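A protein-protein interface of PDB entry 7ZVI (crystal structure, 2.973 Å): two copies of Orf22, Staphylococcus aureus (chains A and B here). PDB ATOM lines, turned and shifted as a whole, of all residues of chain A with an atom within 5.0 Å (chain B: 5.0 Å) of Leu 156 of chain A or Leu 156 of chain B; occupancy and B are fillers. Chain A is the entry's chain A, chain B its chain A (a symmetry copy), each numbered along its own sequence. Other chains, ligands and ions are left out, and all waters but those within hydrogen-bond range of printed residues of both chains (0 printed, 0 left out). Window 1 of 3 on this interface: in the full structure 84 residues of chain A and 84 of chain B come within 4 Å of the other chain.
Among the printed residues, pairs that only touch across the chains: Tyr 150 of chain A with Phe 151 of chain B (3.7 Å), Phe 151 of chain A with Tyr 150 of chain B (3.7 Å), Phe 151 of chain A with Trp 155 of chain B (3.8 Å), Phe 151 of chain A with Leu 156 of chain B (3.95 Å), Phe 151 of chain A with Val 164 of chain B (3.3 Å), Leu 153 of chain A with Leu 153 of chain B (3.7 Å), Leu 153 of chain A with Leu 156 of chain B (3.98 Å), Leu 153 of chain A with Leu 157 of chain B (3.9 Å), Leu 153 of chain A with Val 164 of chain B (3.8 Å), Trp 155 of chain A with Phe 151 of chain B (3.8 Å), Leu 156 of chain A with Phe 151 of chain B (3.95 Å), Leu 156 of chain A with Leu 153 of chain B (3.98 Å), Leu 156 of chain A with Leu 156 of chain B (3.5 Å), Leu 157 of chain A with Leu 153 of chain B (3.9 Å), Val 164 of chain A with Phe 151 of chain B (3.3 Å) and Val 164 of chain A with Leu 153 of chain B (3.8 Å).
The side-chain amide nitrogen (NE2) of Gln 159 of chain A sits close to the backbone carbonyl oxygen (O) of Leu 156 of chain A (3.4 Å).
O of Leu 156 of chain B lies close to NE2 of Gln 159 of chain B, at 3.4 Å.
The backbone carbonyl oxygen of Trp 155 of chain B is in hydrogen-bond range of the side-chain hydroxyl of Thr 158 of chain B, at 3.3 Å.
O of Trp 155 of chain A sits at hydrogen-bond distance from OG1 of Thr 158 of chain A, at 3.3 Å.
Hydrophobic or aromatic side chains of chain B within 4 Å of the printed part of chain A: Tyr 150, Phe 151, Leu 153, Trp 155, Leu 156, Leu 157 and Val 164.
Hydrophobic or aromatic side chains of chain A within 4 Å of the printed part of chain B: Tyr 150, Phe 151, Leu 153, Trp 155, Leu 156, Leu 157 and Val 164.
Among the printed residues, 16 pairs touch across the chains.
Of chain B, only Phe 151, Leu 153 and Leu 156 come within 4 Å of Leu 156 of chain A.
Leu 156 of chain B touches just these residues of chain A: Phe 151 (3.95 Å), Leu 153 (3.98 Å) and Leu 156 (3.5 Å).
Printed residues of chain A within 4 Å of Tyr 150 of chain B: Phe 151 (3.7 Å).
Printed residues of chain B within 4 Å of Leu 157 of chain A: Leu 153.
Of the printed residues of chain B, Tyr 150 of chain A touches Phe 151.
Of the printed residues of chain B, Val 164 of chain A touches Phe 151 and Leu 153.
Of the printed residues of chain A, Leu 157 of chain B touches Leu 153.
Asp 152 of chain B touches none of the printed residues of chain A.
The nearest residue of chain B that does not touch Leu 156 of chain A is Tyr 150 of chain B (4.1 Å).
The nearest printed residue of chain B that does not touch Tyr 150 of chain A is Leu 156 of chain B (4.1 Å).
Phe 151 of chain A touches Leu 156 of chain B, and with the chains exchanged Leu 156 of chain A touches Phe 151 of chain B.
Phe 151 of chain A touches Val 164 of chain B, and with the chains exchanged Val 164 of chain A touches Phe 151 of chain B.
Leu 153 of chain A touches Leu 156 of chain B, and with the chains exchanged Leu 156 of chain A touches Leu 153 of chain B.
Leu 153 of chain A touches Leu 157 of chain B, and with the chains exchanged Leu 157 of chain A touches Leu 153 of chain B.
Of the 16 pairs that touch across the chains among the printed residues, 16 have their exchanged pair printed and touching as well.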
ATOM      1  N   TYR A 150      -5.480 -16.625  -6.903  1.00  0.00           N
ATOM      2  CA  TYR A 150      -6.068 -17.413  -5.786  1.00  0.00           C
ATOM      3  C   TYR A 150      -7.585 -17.198  -5.721  1.00  0.00           C
ATOM      4  O   TYR A 150      -8.300 -18.138  -5.320  1.00  0.00           O
ATOM      5  CB  TYR A 150      -5.436 -17.032  -4.444  1.00  0.00           C
ATOM      6  CG  TYR A 150      -3.958 -17.310  -4.322  1.00  0.00           C
ATOM      7  CD1 TYR A 150      -3.482 -18.599  -4.144  1.00  0.00           C
ATOM      8  CD2 TYR A 150      -3.032 -16.279  -4.355  1.00  0.00           C
ATOM      9  CE1 TYR A 150      -2.126 -18.858  -4.018  1.00  0.00           C
ATOM     10  CE2 TYR A 150      -1.673 -16.520  -4.231  1.00  0.00           C
ATOM     11  CZ  TYR A 150      -1.216 -17.816  -4.060  1.00  0.00           C
ATOM     12  OH  TYR A 150       0.121 -18.068  -3.937  1.00  0.00           O
ATOM     13  N   PHE A 151      -8.054 -16.001  -6.088  1.00  0.00           N
ATOM     14  CA  PHE A 151      -9.469 -15.567  -5.948  1.00  0.00           C
ATOM     15  C   PHE A 151     -10.266 -15.895  -7.217  1.00  0.00           C
ATOM     16  O   PHE A 151     -11.499 -15.771  -7.178  1.00  0.00           O
ATOM     17  CB  PHE A 151      -9.531 -14.080  -5.587  1.00  0.00           C
ATOM     18  CG  PHE A 151      -8.927 -13.768  -4.242  1.00  0.00           C
ATOM     19  CD1 PHE A 151      -9.657 -13.953  -3.076  1.00  0.00           C
ATOM     20  CD2 PHE A 151      -7.618 -13.322  -4.137  1.00  0.00           C
ATOM     21  CE1 PHE A 151      -9.097 -13.679  -1.837  1.00  0.00           C
ATOM     22  CE2 PHE A 151      -7.060 -13.046  -2.897  1.00  0.00           C
ATOM     23  CZ  PHE A 151      -7.799 -13.228  -1.750  1.00  0.00           C
ATOM     24  N   ASP A 152      -9.594 -16.301  -8.297  1.00  0.00           N
ATOM     25  CA  ASP A 152     -10.249 -16.831  -9.523  1.00  0.00           C
ATOM     26  C   ASP A 152     -10.780 -18.234  -9.203  1.00  0.00           C
ATOM     27  O   ASP A 152      -9.956 -19.167  -9.099  1.00  0.00           O
ATOM     28  CB  ASP A 152      -9.293 -16.824 -10.719  1.00  0.00           C
ATOM     29  CG  ASP A 152      -9.935 -17.245 -12.031  1.00  0.00           C
ATOM     30  OD1 ASP A 152     -11.167 -17.445 -12.043  1.00  0.00           O
ATOM     31  OD2 ASP A 152      -9.200 -17.369 -13.033  1.00  0.00           O
ATOM     32  N   LEU A 153     -12.102 -18.360  -9.037  1.00  0.00           N
ATOM     33  CA  LEU A 153     -12.806 -19.632  -8.711  1.00  0.00           C
ATOM     34  C   LEU A 153     -12.459 -20.696  -9.758  1.00  0.00           C
ATOM     35  O   LEU A 153     -12.229 -21.854  -9.363  1.00  0.00           O
ATOM     36  CB  LEU A 153     -14.317 -19.380  -8.665  1.00  0.00           C
ATOM     37  CG  LEU A 153     -15.202 -20.622  -8.534  1.00  0.00           C
ATOM     38  CD1 LEU A 153     -14.823 -21.452  -7.316  1.00  0.00           C
ATOM     39  CD2 LEU A 153     -16.668 -20.227  -8.462  1.00  0.00           C
ATOM     40  N   ASN A 154     -12.435 -20.318 -11.039  1.00  0.00           N
ATOM     41  CA  ASN A 154     -12.134 -21.246 -12.160  1.00  0.00           C
ATOM     42  C   ASN A 154     -10.753 -21.867 -11.943  1.00  0.00           C
ATOM     43  O   ASN A 154     -10.666 -23.107 -11.970  1.00  0.00           O
ATOM     44  CB  ASN A 154     -12.183 -20.564 -13.527  1.00  0.00           C
ATOM     45  CG  ASN A 154     -11.731 -21.498 -14.629  1.00  0.00           C
ATOM     46  OD1 ASN A 154     -12.273 -22.592 -14.777  1.00  0.00           O
ATOM     47  ND2 ASN A 154     -10.726 -21.093 -15.388  1.00  0.00           N
ATOM     48  N   TRP A 155      -9.726 -21.033 -11.739  1.00  0.00           N
ATOM     49  CA  TRP A 155      -8.311 -21.461 -11.560  1.00  0.00           C
ATOM     50  C   TRP A 155      -8.191 -22.439 -10.387  1.00  0.00           C
ATOM     51  O   TRP A 155      -7.495 -23.456 -10.549  1.00  0.00           O
ATOM     52  CB  TRP A 155      -7.372 -20.266 -11.359  1.00  0.00           C
ATOM     53  CG  TRP A 155      -6.014 -20.674 -10.873  1.00  0.00           C
ATOM     54  CD1 TRP A 155      -4.938 -21.025 -11.637  1.00  0.00           C
ATOM     55  CD2 TRP A 155      -5.590 -20.804  -9.505  1.00  0.00           C
ATOM     56  NE1 TRP A 155      -3.875 -21.352 -10.839  1.00  0.00           N
ATOM     57  CE2 TRP A 155      -4.244 -21.229  -9.527  1.00  0.00           C
ATOM     58  CE3 TRP A 155      -6.211 -20.602  -8.267  1.00  0.00           C
ATOM     59  CZ2 TRP A 155      -3.512 -21.448  -8.358  1.00  0.00           C
ATOM     60  CZ3 TRP A 155      -5.489 -20.821  -7.113  1.00  0.00           C
ATOM     61  CH2 TRP A 155      -4.158 -21.237  -7.161  1.00  0.00           C
ATOM     62  N   LEU A 156      -8.811 -22.125  -9.244  1.00  0.00           N
ATOM     63  CA  LEU A 156      -8.745 -22.965  -8.017  1.00  0.00           C
ATOM     64  C   LEU A 156      -9.192 -24.390  -8.361  1.00  0.00           C
ATOM     65  O   LEU A 156      -8.530 -25.339  -7.900  1.00  0.00           O
ATOM     66  CB  LEU A 156      -9.625 -22.362  -6.914  1.00  0.00           C
ATOM     67  CG  LEU A 156      -9.769 -23.210  -5.648  1.00  0.00           C
ATOM     68  CD1 LEU A 156      -8.411 -23.560  -5.060  1.00  0.00           C
ATOM     69  CD2 LEU A 156     -10.618 -22.503  -4.609  1.00  0.00           C
ATOM     70  N   LEU A 157     -10.263 -24.519  -9.151  1.00  0.00           N
ATOM     71  CA  LEU A 157     -10.912 -25.814  -9.495  1.00  0.00           C
ATOM     72  C   LEU A 157     -10.100 -26.557 -10.566  1.00  0.00           C
ATOM     73  O   LEU A 157     -10.164 -27.797 -10.571  1.00  0.00           O
ATOM     74  CB  LEU A 157     -12.348 -25.553  -9.970  1.00  0.00           C
ATOM     75  CG  LEU A 157     -13.310 -24.991  -8.921  1.00  0.00           C
ATOM     76  CD1 LEU A 157     -14.635 -24.594  -9.552  1.00  0.00           C
ATOM     77  CD2 LEU A 157     -13.544 -25.985  -7.795  1.00  0.00           C
ATOM     78  N   THR A 158      -9.361 -25.847 -11.428  1.00  0.00           N
ATOM     79  CA  THR A 158      -8.677 -26.435 -12.614  1.00  0.00           C
ATOM     80  C   THR A 158      -7.188 -26.706 -12.346  1.00  0.00           C
ATOM     81  O   THR A 158      -6.657 -27.624 -12.994  1.00  0.00           O
ATOM     82  CB  THR A 158      -8.864 -25.559 -13.859  1.00  0.00           C
ATOM     83  OG1 THR A 158      -8.240 -24.292 -13.651  1.00  0.00           O
ATOM     84  CG2 THR A 158     -10.322 -25.355 -14.210  1.00  0.00           C
ATOM     85  N   GLN A 159      -6.533 -25.954 -11.452  1.00  0.00           N
ATOM     86  CA  GLN A 159      -5.069 -26.077 -11.179  1.00  0.00           C
ATOM     87  C   GLN A 159      -4.748 -27.478 -10.631  1.00  0.00           C
ATOM     88  O   GLN A 159      -5.653 -28.113 -10.045  1.00  0.00           O
ATOM     89  CB  GLN A 159      -4.581 -24.973 -10.232  1.00  0.00           C
ATOM     90  CG  GLN A 159      -5.259 -24.954  -8.864  1.00  0.00           C
ATOM     91  CD  GLN A 159      -4.667 -25.906  -7.850  1.00  0.00           C
ATOM     92  OE1 GLN A 159      -3.586 -26.461  -8.035  1.00  0.00           O
ATOM     93  NE2 GLN A 159      -5.377 -26.091  -6.749  1.00  0.00           N
ATOM     94  N   VAL A 164      -7.118 -28.980  -2.988  1.00  0.00           N
ATOM     95  CA  VAL A 164      -8.263 -28.087  -2.641  1.00  0.00           C
ATOM     96  C   VAL A 164      -9.060 -28.762  -1.523  1.00  0.00           C
ATOM     97  O   VAL A 164      -9.256 -29.983  -1.601  1.00  0.00           O
ATOM     98  CB  VAL A 164      -9.139 -27.801  -3.875  1.00  0.00           C
ATOM     99  CG1 VAL A 164     -10.388 -27.006  -3.524  1.00  0.00           C
ATOM    100  CG2 VAL A 164      -8.344 -27.102  -4.966  1.00  0.00           C
ATOM    101  N   TYR B 150      -6.766 -19.959   1.296  1.00  0.00           N
ATOM    102  CA  TYR B 150      -7.017 -19.595  -0.125  1.00  0.00           C
ATOM    103  C   TYR B 150      -7.498 -20.819  -0.913  1.00  0.00           C
ATOM    104  O   TYR B 150      -8.289 -20.641  -1.859  1.00  0.00           O
ATOM    105  CB  TYR B 150      -5.759 -19.020  -0.781  1.00  0.00           C
ATOM    106  CG  TYR B 150      -5.243 -17.736  -0.181  1.00  0.00           C
ATOM    107  CD1 TYR B 150      -5.879 -16.527  -0.417  1.00  0.00           C
ATOM    108  CD2 TYR B 150      -4.100 -17.721   0.601  1.00  0.00           C
ATOM    109  CE1 TYR B 150      -5.402 -15.342   0.121  1.00  0.00           C
ATOM    110  CE2 TYR B 150      -3.609 -16.545   1.148  1.00  0.00           C
ATOM    111  CZ  TYR B 150      -4.262 -15.348   0.906  1.00  0.00           C
ATOM    112  OH  TYR B 150      -3.789 -14.182   1.438  1.00  0.00           O
ATOM    113  N   PHE B 151      -7.024 -22.014  -0.544  1.00  0.00           N
ATOM    114  CA  PHE B 151      -7.261 -23.283  -1.283  1.00  0.00           C
ATOM    115  C   PHE B 151      -8.516 -23.991  -0.757  1.00  0.00           C
ATOM    116  O   PHE B 151      -8.951 -24.958  -1.400  1.00  0.00           O
ATOM    117  CB  PHE B 151      -6.016 -24.171  -1.215  1.00  0.00           C
ATOM    118  CG  PHE B 151      -4.819 -23.574  -1.908  1.00  0.00           C
ATOM    119  CD1 PHE B 151      -4.667 -23.681  -3.283  1.00  0.00           C
ATOM    120  CD2 PHE B 151      -3.859 -22.874  -1.191  1.00  0.00           C
ATOM    121  CE1 PHE B 151      -3.572 -23.119  -3.922  1.00  0.00           C
ATOM    122  CE2 PHE B 151      -2.764 -22.314  -1.832  1.00  0.00           C
ATOM    123  CZ  PHE B 151      -2.623 -22.435  -3.195  1.00  0.00           C
ATOM    124  N   ASP B 152      -9.078 -23.530   0.363  1.00  0.00           N
ATOM    125  CA  ASP B 152     -10.395 -23.996   0.874  1.00  0.00           C
ATOM    126  C   ASP B 152     -11.486 -23.412  -0.033  1.00  0.00           C
ATOM    127  O   ASP B 152     -11.747 -22.195   0.067  1.00  0.00           O
ATOM    128  CB  ASP B 152     -10.592 -23.620   2.346  1.00  0.00           C
ATOM    129  CG  ASP B 152     -11.869 -24.168   2.962  1.00  0.00           C
ATOM    130  OD1 ASP B 152     -12.566 -24.943   2.276  1.00  0.00           O
ATOM    131  OD2 ASP B 152     -12.157 -23.818   4.126  1.00  0.00           O
ATOM    132  N   LEU B 153     -12.076 -24.253  -0.892  1.00  0.00           N
ATOM    133  CA  LEU B 153     -13.144 -23.876  -1.859  1.00  0.00           C
ATOM    134  C   LEU B 153     -14.313 -23.227  -1.111  1.00  0.00           C
ATOM    135  O   LEU B 153     -14.849 -22.223  -1.616  1.00  0.00           O
ATOM    136  CB  LEU B 153     -13.605 -25.124  -2.621  1.00  0.00           C
ATOM    137  CG  LEU B 153     -14.833 -24.950  -3.517  1.00  0.00           C
ATOM    138  CD1 LEU B 153     -14.634 -23.828  -4.525  1.00  0.00           C
ATOM    139  CD2 LEU B 153     -15.156 -26.249  -4.237  1.00  0.00           C
ATOM    140  N   ASN B 154     -14.697 -23.787   0.040  1.00  0.00           N
ATOM    141  CA  ASN B 154     -15.825 -23.277   0.862  1.00  0.00           C
ATOM    142  C   ASN B 154     -15.554 -21.821   1.243  1.00  0.00           C
ATOM    143  O   ASN B 154     -16.432 -20.981   0.983  1.00  0.00           O
ATOM    144  CB  ASN B 154     -16.064 -24.105   2.124  1.00  0.00           C
ATOM    145  CG  ASN B 154     -17.121 -23.476   3.007  1.00  0.00           C
ATOM    146  OD1 ASN B 154     -18.235 -23.219   2.555  1.00  0.00           O
ATOM    147  ND2 ASN B 154     -16.778 -23.200   4.255  1.00  0.00           N
ATOM    148  N   TRP B 155     -14.384 -21.545   1.834  1.00  0.00           N
ATOM    149  CA  TRP B 155     -13.977 -20.196   2.316  1.00  0.00           C
ATOM    150  C   TRP B 155     -14.023 -19.182   1.169  1.00  0.00           C
ATOM    151  O   TRP B 155     -14.541 -18.075   1.396  1.00  0.00           O
ATOM    152  CB  TRP B 155     -12.585 -20.215   2.959  1.00  0.00           C
ATOM    153  CG  TRP B 155     -12.028 -18.839   3.168  1.00  0.00           C
ATOM    154  CD1 TRP B 155     -12.207 -18.034   4.256  1.00  0.00           C
ATOM    155  CD2 TRP B 155     -11.220 -18.086   2.245  1.00  0.00           C
ATOM    156  NE1 TRP B 155     -11.558 -16.842   4.079  1.00  0.00           N
ATOM    157  CE2 TRP B 155     -10.946 -16.842   2.854  1.00  0.00           C
ATOM    158  CE3 TRP B 155     -10.701 -18.340   0.971  1.00  0.00           C
ATOM    159  CZ2 TRP B 155     -10.171 -15.862   2.232  1.00  0.00           C
ATOM    160  CZ3 TRP B 155      -9.938 -17.371   0.355  1.00  0.00           C
ATOM    161  CH2 TRP B 155      -9.677 -16.150   0.979  1.00  0.00           C
ATOM    162  N   LEU B 156     -13.472 -19.530   0.002  1.00  0.00           N
ATOM    163  CA  LEU B 156     -13.414 -18.627  -1.180  1.00  0.00           C
ATOM    164  C   LEU B 156     -14.830 -18.143  -1.511  1.00  0.00           C
ATOM    165  O   LEU B 156     -14.987 -16.940  -1.789  1.00  0.00           O
ATOM    166  CB  LEU B 156     -12.787 -19.358  -2.375  1.00  0.00           C
ATOM    167  CG  LEU B 156     -12.808 -18.593  -3.700  1.00  0.00           C
ATOM    168  CD1 LEU B 156     -12.154 -17.227  -3.560  1.00  0.00           C
ATOM    169  CD2 LEU B 156     -12.124 -19.385  -4.800  1.00  0.00           C
ATOM    170  N   LEU B 157     -15.811 -19.051  -1.465  1.00  0.00           N
ATOM    171  CA  LEU B 157     -17.221 -18.797  -1.866  1.00  0.00           C
ATOM    172  C   LEU B 157     -17.963 -18.018  -0.770  1.00  0.00           C
ATOM    173  O   LEU B 157     -18.898 -17.283  -1.126  1.00  0.00           O
ATOM    174  CB  LEU B 157     -17.914 -20.134  -2.163  1.00  0.00           C
ATOM    175  CG  LEU B 157     -17.382 -20.913  -3.368  1.00  0.00           C
ATOM    176  CD1 LEU B 157     -18.009 -22.296  -3.443  1.00  0.00           C
ATOM    177  CD2 LEU B 157     -17.622 -20.158  -4.666  1.00  0.00           C
ATOM    178  N   THR B 158     -17.569 -18.156   0.502  1.00  0.00           N
ATOM    179  CA  THR B 158     -18.314 -17.599   1.666  1.00  0.00           C
ATOM    180  C   THR B 158     -17.713 -16.272   2.155  1.00  0.00           C
ATOM    181  O   THR B 158     -18.486 -15.476   2.716  1.00  0.00           O
ATOM    182  CB  THR B 158     -18.409 -18.618   2.809  1.00  0.00           C
ATOM    183  OG1 THR B 158     -17.102 -18.908   3.301  1.00  0.00           O
ATOM    184  CG2 THR B 158     -19.089 -19.902   2.385  1.00  0.00           C
ATOM    185  N   GLN B 159     -16.408 -16.034   1.971  1.00  0.00           N
ATOM    186  CA  GLN B 159     -15.707 -14.816   2.482  1.00  0.00           C
ATOM    187  C   GLN B 159     -16.300 -13.553   1.836  1.00  0.00           C
ATOM    188  O   GLN B 159     -16.857 -13.657   0.721  1.00  0.00           O
ATOM    189  CB  GLN B 159     -14.192 -14.909   2.261  1.00  0.00           C
ATOM    190  CG  GLN B 159     -13.763 -15.054   0.803  1.00  0.00           C
ATOM    191  CD  GLN B 159     -13.665 -13.753   0.039  1.00  0.00           C
ATOM    192  OE1 GLN B 159     -13.688 -12.663   0.607  1.00  0.00           O
ATOM    193  NE2 GLN B 159     -13.539 -13.863  -1.274  1.00  0.00           N
ATOM    194  N   VAL B 164     -14.450 -12.313  -5.995  1.00  0.00           N
ATOM    195  CA  VAL B 164     -14.124 -13.621  -6.638  1.00  0.00           C
ATOM    196  C   VAL B 164     -14.384 -13.480  -8.140  1.00  0.00           C
ATOM    197  O   VAL B 164     -15.401 -12.872  -8.502  1.00  0.00           O
ATOM    198  CB  VAL B 164     -14.948 -14.765  -6.021  1.00  0.00           C
ATOM    199  CG1 VAL B 164     -14.738 -16.086  -6.748  1.00  0.00           C
ATOM    200  CG2 VAL B 164     -14.657 -14.916  -4.536  1.00  0.00           C
